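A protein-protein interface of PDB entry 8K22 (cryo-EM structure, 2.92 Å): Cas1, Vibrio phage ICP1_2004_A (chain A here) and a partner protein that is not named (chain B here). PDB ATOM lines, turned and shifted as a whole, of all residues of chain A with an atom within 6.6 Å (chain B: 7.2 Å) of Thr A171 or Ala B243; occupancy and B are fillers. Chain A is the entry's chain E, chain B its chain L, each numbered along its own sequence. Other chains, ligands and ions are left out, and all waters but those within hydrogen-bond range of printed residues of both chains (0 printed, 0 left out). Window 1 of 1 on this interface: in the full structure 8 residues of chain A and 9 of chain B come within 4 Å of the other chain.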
ATOM      1  N   ILE A 148       8.553  10.110   5.489  1.00  0.00           N
ATOM      2  CA  ILE A 148       9.989  10.365   5.597  1.00  0.00           C
ATOM      3  C   ILE A 148      10.788   9.115   5.230  1.00  0.00           C
ATOM      4  O   ILE A 148      11.808   9.193   4.530  1.00  0.00           O
ATOM      5  CB  ILE A 148      10.324  10.871   7.015  1.00  0.00           C
ATOM      6  CG1 ILE A 148       9.714  12.253   7.240  1.00  0.00           C
ATOM      7  CG2 ILE A 148      11.818  10.945   7.250  1.00  0.00           C
ATOM      8  CD1 ILE A 148       9.829  12.743   8.665  1.00  0.00           C
ATOM      9  N   LYS A 151      10.550   8.643   1.472  1.00  0.00           N
ATOM     10  CA  LYS A 151      11.389   9.657   0.842  1.00  0.00           C
ATOM     11  C   LYS A 151      12.857   9.259   0.894  1.00  0.00           C
ATOM     12  O   LYS A 151      13.573   9.368  -0.110  1.00  0.00           O
ATOM     13  CB  LYS A 151      11.182  11.005   1.528  1.00  0.00           C
ATOM     14  CG  LYS A 151      12.146  12.093   1.070  1.00  0.00           C
ATOM     15  CD  LYS A 151      11.450  13.425   0.803  1.00  0.00           C
ATOM     16  CE  LYS A 151      10.407  13.757   1.863  1.00  0.00           C
ATOM     17  NZ  LYS A 151      11.023  14.056   3.184  1.00  0.00           N
ATOM     18  N   PHE A 152      13.308   8.761   2.049  1.00  0.00           N
ATOM     19  CA  PHE A 152      14.682   8.290   2.186  1.00  0.00           C
ATOM     20  C   PHE A 152      14.943   7.070   1.309  1.00  0.00           C
ATOM     21  O   PHE A 152      16.016   6.950   0.713  1.00  0.00           O
ATOM     22  CB  PHE A 152      14.979   7.968   3.647  1.00  0.00           C
ATOM     23  CG  PHE A 152      16.436   7.805   3.945  1.00  0.00           C
ATOM     24  CD1 PHE A 152      17.370   8.657   3.377  1.00  0.00           C
ATOM     25  CD2 PHE A 152      16.876   6.798   4.788  1.00  0.00           C
ATOM     26  CE1 PHE A 152      18.714   8.514   3.654  1.00  0.00           C
ATOM     27  CE2 PHE A 152      18.218   6.647   5.065  1.00  0.00           C
ATOM     28  CZ  PHE A 152      19.139   7.505   4.497  1.00  0.00           C
ATOM     29  N   LEU A 166      24.857  11.677   1.230  1.00  0.00           N
ATOM     30  CA  LEU A 166      25.084  12.480   2.432  1.00  0.00           C
ATOM     31  C   LEU A 166      23.984  13.513   2.635  1.00  0.00           C
ATOM     32  O   LEU A 166      23.514  13.703   3.764  1.00  0.00           O
ATOM     33  CB  LEU A 166      26.447  13.175   2.383  1.00  0.00           C
ATOM     34  CG  LEU A 166      27.723  12.518   2.924  1.00  0.00           C
ATOM     35  CD1 LEU A 166      27.725  12.610   4.442  1.00  0.00           C
ATOM     36  CD2 LEU A 166      27.897  11.083   2.500  1.00  0.00           C
ATOM     37  N   GLY A 167      23.571  14.192   1.561  1.00  0.00           N
ATOM     38  CA  GLY A 167      22.464  15.132   1.674  1.00  0.00           C
ATOM     39  C   GLY A 167      21.162  14.454   2.062  1.00  0.00           C
ATOM     40  O   GLY A 167      20.417  14.953   2.910  1.00  0.00           O
ATOM     41  N   HIS A 168      20.905  13.278   1.487  1.00  0.00           N
ATOM     42  CA  HIS A 168      19.691  12.531   1.799  1.00  0.00           C
ATOM     43  C   HIS A 168      19.727  11.957   3.211  1.00  0.00           C
ATOM     44  O   HIS A 168      18.694  11.925   3.893  1.00  0.00           O
ATOM     45  CB  HIS A 168      19.512  11.428   0.762  1.00  0.00           C
ATOM     46  CG  HIS A 168      19.196  11.936  -0.611  1.00  0.00           C
ATOM     47  ND1 HIS A 168      18.717  11.118  -1.608  1.00  0.00           N
ATOM     48  CD2 HIS A 168      19.246  13.181  -1.142  1.00  0.00           C
ATOM     49  CE1 HIS A 168      18.514  11.829  -2.703  1.00  0.00           C
ATOM     50  NE2 HIS A 168      18.827  13.086  -2.447  1.00  0.00           N
ATOM     51  N   GLU A 169      20.904  11.523   3.667  1.00  0.00           N
ATOM     52  CA  GLU A 169      21.067  11.030   5.030  1.00  0.00           C
ATOM     53  C   GLU A 169      20.859  12.146   6.041  1.00  0.00           C
ATOM     54  O   GLU A 169      20.207  11.945   7.070  1.00  0.00           O
ATOM     55  CB  GLU A 169      22.449  10.368   5.164  1.00  0.00           C
ATOM     56  CG  GLU A 169      23.116  10.270   6.558  1.00  0.00           C
ATOM     57  CD  GLU A 169      23.841  11.525   7.034  1.00  0.00           C
ATOM     58  OE1 GLU A 169      24.276  12.324   6.182  1.00  0.00           O
ATOM     59  OE2 GLU A 169      23.971  11.704   8.263  1.00  0.00           O
ATOM     60  N   GLY A 170      21.418  13.328   5.765  1.00  0.00           N
ATOM     61  CA  GLY A 170      21.207  14.461   6.651  1.00  0.00           C
ATOM     62  C   GLY A 170      19.758  14.904   6.683  1.00  0.00           C
ATOM     63  O   GLY A 170      19.230  15.247   7.747  1.00  0.00           O
ATOM     64  N   THR A 171      19.091  14.862   5.524  1.00  0.00           N
ATOM     65  CA  THR A 171      17.670  15.181   5.444  1.00  0.00           C
ATOM     66  C   THR A 171      16.840  14.204   6.269  1.00  0.00           C
ATOM     67  O   THR A 171      15.987  14.621   7.057  1.00  0.00           O
ATOM     68  CB  THR A 171      17.230  15.186   3.976  1.00  0.00           C
ATOM     69  OG1 THR A 171      17.666  16.401   3.355  1.00  0.00           O
ATOM     70  CG2 THR A 171      15.716  15.084   3.842  1.00  0.00           C
ATOM     71  N   PHE A 172      17.132  12.903   6.158  1.00  0.00           N
ATOM     72  CA  PHE A 172      16.399  11.893   6.923  1.00  0.00           C
ATOM     73  C   PHE A 172      16.652  12.011   8.422  1.00  0.00           C
ATOM     74  O   PHE A 172      15.709  11.928   9.222  1.00  0.00           O
ATOM     75  CB  PHE A 172      16.776  10.495   6.434  1.00  0.00           C
ATOM     76  CG  PHE A 172      16.254   9.384   7.301  1.00  0.00           C
ATOM     77  CD1 PHE A 172      14.912   9.050   7.287  1.00  0.00           C
ATOM     78  CD2 PHE A 172      17.113   8.656   8.110  1.00  0.00           C
ATOM     79  CE1 PHE A 172      14.429   8.026   8.078  1.00  0.00           C
ATOM     80  CE2 PHE A 172      16.635   7.630   8.902  1.00  0.00           C
ATOM     81  CZ  PHE A 172      15.293   7.315   8.883  1.00  0.00           C
ATOM     82  N   VAL A 173      17.912  12.218   8.817  1.00  0.00           N
ATOM     83  CA  VAL A 173      18.276  12.258  10.230  1.00  0.00           C
ATOM     84  C   VAL A 173      17.664  13.479  10.902  1.00  0.00           C
ATOM     85  O   VAL A 173      17.024  13.378  11.958  1.00  0.00           O
ATOM     86  CB  VAL A 173      19.809  12.237  10.377  1.00  0.00           C
ATOM     87  CG1 VAL A 173      20.250  12.762  11.731  1.00  0.00           C
ATOM     88  CG2 VAL A 173      20.334  10.847  10.161  1.00  0.00           C
ATOM     89  N   LYS A 174      17.803  14.645  10.276  1.00  0.00           N
ATOM     90  CA  LYS A 174      17.262  15.850  10.880  1.00  0.00           C
ATOM     91  C   LYS A 174      15.745  15.918  10.701  1.00  0.00           C
ATOM     92  O   LYS A 174      15.057  16.557  11.500  1.00  0.00           O
ATOM     93  CB  LYS A 174      17.994  17.048  10.279  1.00  0.00           C
ATOM     94  CG  LYS A 174      17.319  18.400  10.363  1.00  0.00           C
ATOM     95  CD  LYS A 174      17.720  19.223   9.186  1.00  0.00           C
ATOM     96  CE  LYS A 174      17.289  18.437   7.962  1.00  0.00           C
ATOM     97  NZ  LYS A 174      16.965  19.261   6.845  1.00  0.00           N
ATOM     98  N   SER A 175      15.186  15.194   9.726  1.00  0.00           N
ATOM     99  CA  SER A 175      13.734  15.096   9.626  1.00  0.00           C
ATOM    100  C   SER A 175      13.162  14.254  10.757  1.00  0.00           C
ATOM    101  O   SER A 175      12.094  14.569  11.294  1.00  0.00           O
ATOM    102  CB  SER A 175      13.339  14.516   8.270  1.00  0.00           C
ATOM    103  OG  SER A 175      13.750  15.370   7.217  1.00  0.00           O
ATOM    104  N   LEU A 176      13.866  13.189  11.147  1.00  0.00           N
ATOM    105  CA  LEU A 176      13.462  12.457  12.343  1.00  0.00           C
ATOM    106  C   LEU A 176      13.674  13.287  13.604  1.00  0.00           C
ATOM    107  O   LEU A 176      12.888  13.176  14.554  1.00  0.00           O
ATOM    108  CB  LEU A 176      14.221  11.136  12.439  1.00  0.00           C
ATOM    109  CG  LEU A 176      13.619   9.953  11.682  1.00  0.00           C
ATOM    110  CD1 LEU A 176      14.234   8.671  12.189  1.00  0.00           C
ATOM    111  CD2 LEU A 176      12.106   9.905  11.823  1.00  0.00           C
ATOM    112  N   ASP B 237      13.463  23.024  -4.569  1.00  0.00           N
ATOM    113  CA  ASP B 237      14.793  22.969  -3.963  1.00  0.00           C
ATOM    114  C   ASP B 237      14.753  22.169  -2.669  1.00  0.00           C
ATOM    115  O   ASP B 237      14.401  22.690  -1.610  1.00  0.00           O
ATOM    116  CB  ASP B 237      15.309  24.379  -3.704  1.00  0.00           C
ATOM    117  CG  ASP B 237      16.782  24.525  -3.993  1.00  0.00           C
ATOM    118  OD1 ASP B 237      17.457  23.495  -4.182  1.00  0.00           O
ATOM    119  OD2 ASP B 237      17.267  25.673  -4.022  1.00  0.00           O
ATOM    120  N   THR B 238      15.121  20.891  -2.753  1.00  0.00           N
ATOM    121  CA  THR B 238      15.330  20.053  -1.578  1.00  0.00           C
ATOM    122  C   THR B 238      16.777  19.593  -1.475  1.00  0.00           C
ATOM    123  O   THR B 238      17.050  18.556  -0.865  1.00  0.00           O
ATOM    124  CB  THR B 238      14.406  18.835  -1.601  1.00  0.00           C
ATOM    125  OG1 THR B 238      14.705  18.033  -2.749  1.00  0.00           O
ATOM    126  CG2 THR B 238      12.957  19.260  -1.655  1.00  0.00           C
ATOM    127  N   TRP B 239      17.712  20.332  -2.073  1.00  0.00           N
ATOM    128  CA  TRP B 239      19.084  19.864  -2.212  1.00  0.00           C
ATOM    129  C   TRP B 239      20.110  20.784  -1.568  1.00  0.00           C
ATOM    130  O   TRP B 239      21.314  20.585  -1.768  1.00  0.00           O
ATOM    131  CB  TRP B 239      19.421  19.661  -3.690  1.00  0.00           C
ATOM    132  CG  TRP B 239      18.256  19.190  -4.487  1.00  0.00           C
ATOM    133  CD1 TRP B 239      17.579  18.017  -4.332  1.00  0.00           C
ATOM    134  CD2 TRP B 239      17.631  19.873  -5.575  1.00  0.00           C
ATOM    135  NE1 TRP B 239      16.561  17.934  -5.248  1.00  0.00           N
ATOM    136  CE2 TRP B 239      16.576  19.060  -6.026  1.00  0.00           C
ATOM    137  CE3 TRP B 239      17.862  21.093  -6.212  1.00  0.00           C
ATOM    138  CZ2 TRP B 239      15.748  19.435  -7.075  1.00  0.00           C
ATOM    139  CZ3 TRP B 239      17.041  21.460  -7.256  1.00  0.00           C
ATOM    140  CH2 TRP B 239      16.004  20.630  -7.684  1.00  0.00           C
ATOM    141  N   TYR B 240      19.679  21.781  -0.807  1.00  0.00           N
ATOM    142  CA  TYR B 240      20.609  22.573  -0.025  1.00  0.00           C
ATOM    143  C   TYR B 240      20.940  21.807   1.255  1.00  0.00           C
ATOM    144  O   TYR B 240      20.302  20.805   1.582  1.00  0.00           O
ATOM    145  CB  TYR B 240      20.025  23.959   0.256  1.00  0.00           C
ATOM    146  CG  TYR B 240      18.665  23.988   0.927  1.00  0.00           C
ATOM    147  CD1 TYR B 240      17.485  23.842   0.203  1.00  0.00           C
ATOM    148  CD2 TYR B 240      18.568  24.173   2.293  1.00  0.00           C
ATOM    149  CE1 TYR B 240      16.256  23.866   0.833  1.00  0.00           C
ATOM    150  CE2 TYR B 240      17.351  24.222   2.920  1.00  0.00           C
ATOM    151  CZ  TYR B 240      16.201  24.055   2.193  1.00  0.00           C
ATOM    152  OH  TYR B 240      14.997  24.087   2.850  1.00  0.00           O
ATOM    153  N   GLU B 241      21.969  22.239   1.979  1.00  0.00           N
ATOM    154  CA  GLU B 241      22.272  21.582   3.245  1.00  0.00           C
ATOM    155  C   GLU B 241      21.229  21.996   4.269  1.00  0.00           C
ATOM    156  O   GLU B 241      20.802  23.154   4.290  1.00  0.00           O
ATOM    157  CB  GLU B 241      23.674  21.922   3.767  1.00  0.00           C
ATOM    158  CG  GLU B 241      24.086  23.396   3.982  1.00  0.00           C
ATOM    159  CD  GLU B 241      24.259  24.243   2.733  1.00  0.00           C
ATOM    160  OE1 GLU B 241      23.436  24.174   1.796  1.00  0.00           O
ATOM    161  OE2 GLU B 241      25.267  24.972   2.696  1.00  0.00           O
ATOM    162  N   ASP B 242      20.832  21.036   5.110  1.00  0.00           N
ATOM    163  CA  ASP B 242      19.697  21.135   6.028  1.00  0.00           C
ATOM    164  C   ASP B 242      18.416  21.482   5.260  1.00  0.00           C
ATOM    165  O   ASP B 242      17.742  22.478   5.521  1.00  0.00           O
ATOM    166  CB  ASP B 242      19.967  22.142   7.160  1.00  0.00           C
ATOM    167  CG  ASP B 242      21.182  21.775   7.994  1.00  0.00           C
ATOM    168  OD1 ASP B 242      21.030  20.998   8.958  1.00  0.00           O
ATOM    169  OD2 ASP B 242      22.288  22.267   7.682  1.00  0.00           O
ATOM    170  N   ALA B 243      18.084  20.594   4.317  1.00  0.00           N
ATOM    171  CA  ALA B 243      16.887  20.744   3.496  1.00  0.00           C
ATOM    172  C   ALA B 243      15.715  20.012   4.133  1.00  0.00           C
ATOM    173  O   ALA B 243      15.688  18.778   4.160  1.00  0.00           O
ATOM    174  CB  ALA B 243      17.127  20.214   2.087  1.00  0.00           C
ATOM    175  N   THR B 244      14.748  20.768   4.644  1.00  0.00           N
ATOM    176  CA  THR B 244      13.592  20.200   5.321  1.00  0.00           C
ATOM    177  C   THR B 244      12.373  20.188   4.409  1.00  0.00           C
ATOM    178  O   THR B 244      11.709  19.159   4.261  1.00  0.00           O
ATOM    179  CB  THR B 244      13.276  20.982   6.604  1.00  0.00           C
ATOM    180  OG1 THR B 244      12.388  22.063   6.294  1.00  0.00           O
ATOM    181  CG2 THR B 244      14.542  21.560   7.214  1.00  0.00           C
ATOM    182  N   THR B 245      12.073  21.320   3.784  1.00  0.00           N
ATOM    183  CA  THR B 245      10.955  21.506   2.885  1.00  0.00           C
ATOM    184  C   THR B 245      11.463  22.057   1.558  1.00  0.00           C
ATOM    185  O   THR B 245      12.525  22.685   1.517  1.00  0.00           O
ATOM    186  CB  THR B 245       9.926  22.467   3.503  1.00  0.00           C
ATOM    187  OG1 THR B 245       8.924  22.814   2.541  1.00  0.00           O
ATOM    188  CG2 THR B 245      10.603  23.733   4.004  1.00  0.00           C
ATOM    189  N   PRO B 246      10.768  21.789   0.451  1.00  0.00           N
ATOM    190  CA  PRO B 246      11.138  22.429  -0.816  1.00  0.00           C
ATOM    191  C   PRO B 246      10.927  23.933  -0.759  1.00  0.00           C
ATOM    192  O   PRO B 246       9.841  24.413  -0.430  1.00  0.00           O
ATOM    193  CB  PRO B 246      10.203  21.767  -1.838  1.00  0.00           C
ATOM    194  CG  PRO B 246       9.145  21.090  -1.026  1.00  0.00           C
ATOM    195  CD  PRO B 246       9.824  20.683   0.235  1.00  0.00           C
ATOM    196  N   ILE B 247      11.990  24.672  -1.052  1.00  0.00           N
ATOM    197  CA  ILE B 247      11.933  26.118  -1.169  1.00  0.00           C
ATOM    198  C   ILE B 247      11.996  26.492  -2.645  1.00  0.00           C
ATOM    199  O   ILE B 247      12.313  25.672  -3.505  1.00  0.00           O
ATOM    200  CB  ILE B 247      13.049  26.808  -0.361  1.00  0.00           C
ATOM    201  CG1 ILE B 247      14.337  26.909  -1.183  1.00  0.00           C
ATOM    202  CG2 ILE B 247      13.278  26.091   0.941  1.00  0.00           C
ATOM    203  CD1 ILE B 247      15.279  27.957  -0.708  1.00  0.00           C
ATOM    204  N   TYR B 262      19.020  30.111   2.798  1.00  0.00           N
ATOM    205  CA  TYR B 262      19.528  28.763   3.018  1.00  0.00           C
ATOM    206  C   TYR B 262      20.788  28.434   2.230  1.00  0.00           C
ATOM    207  O   TYR B 262      21.447  27.442   2.549  1.00  0.00           O
ATOM    208  CB  TYR B 262      18.449  27.731   2.690  1.00  0.00           C
ATOM    209  CG  TYR B 262      17.167  27.894   3.464  1.00  0.00           C
ATOM    210  CD1 TYR B 262      17.153  27.774   4.844  1.00  0.00           C
ATOM    211  CD2 TYR B 262      15.965  28.115   2.815  1.00  0.00           C
ATOM    212  CE1 TYR B 262      15.983  27.899   5.558  1.00  0.00           C
ATOM    213  CE2 TYR B 262      14.788  28.247   3.520  1.00  0.00           C
ATOM    214  CZ  TYR B 262      14.803  28.139   4.892  1.00  0.00           C
ATOM    215  OH  TYR B 262      13.631  28.268   5.599  1.00  0.00           O
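The side-chain hydroxyl (OG1) of Thr A171 is in hydrogen-bond range of the backbone carbonyl oxygen (O) of Ala B243 (3.2 Å). The backbone NH (N) of Thr B244 sits close to the side-chain amino group (NZ) of Lys A174, at 3.5 Å. The side-chain amino group of Lys A174 is in hydrogen-bond range of the backbone carbonyl oxygen of Ala B243 (3.0 Å).
O of Gly A167 is in hydrogen-bond range of OG1 of Thr A171, at 3.1 Å.
Among the printed residues, pairs that only touch across the chains: Lys A174 with Asp B242 (3.1 Å).
Of the printed residues of chain B, Thr A171 touches Ala B243 (3.2 Å). Of the printed residues of chain B, Lys A174 touches Asp B242 (3.1 Å), Ala B243 (3.0 Å) and Thr B244 (3.4 Å). Ala B243 touches just these residues of chain A: Thr A171 and Lys A174. Printed residues of chain A within 4 Å of Thr B244: Lys A174 (3.4 Å). Tyr B262 touches none of the printed residues of chain A.
Of the 14 printed residues of chain A, 2 touch a printed residue of chain B. Of the 12 printed residues of chain B, 3 touch a printed residue of chain A. Along chain B the printed residues that touch a printed residue of chain A span positions 242 to 244. Among the printed residues, 4 pairs touch across the chains.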
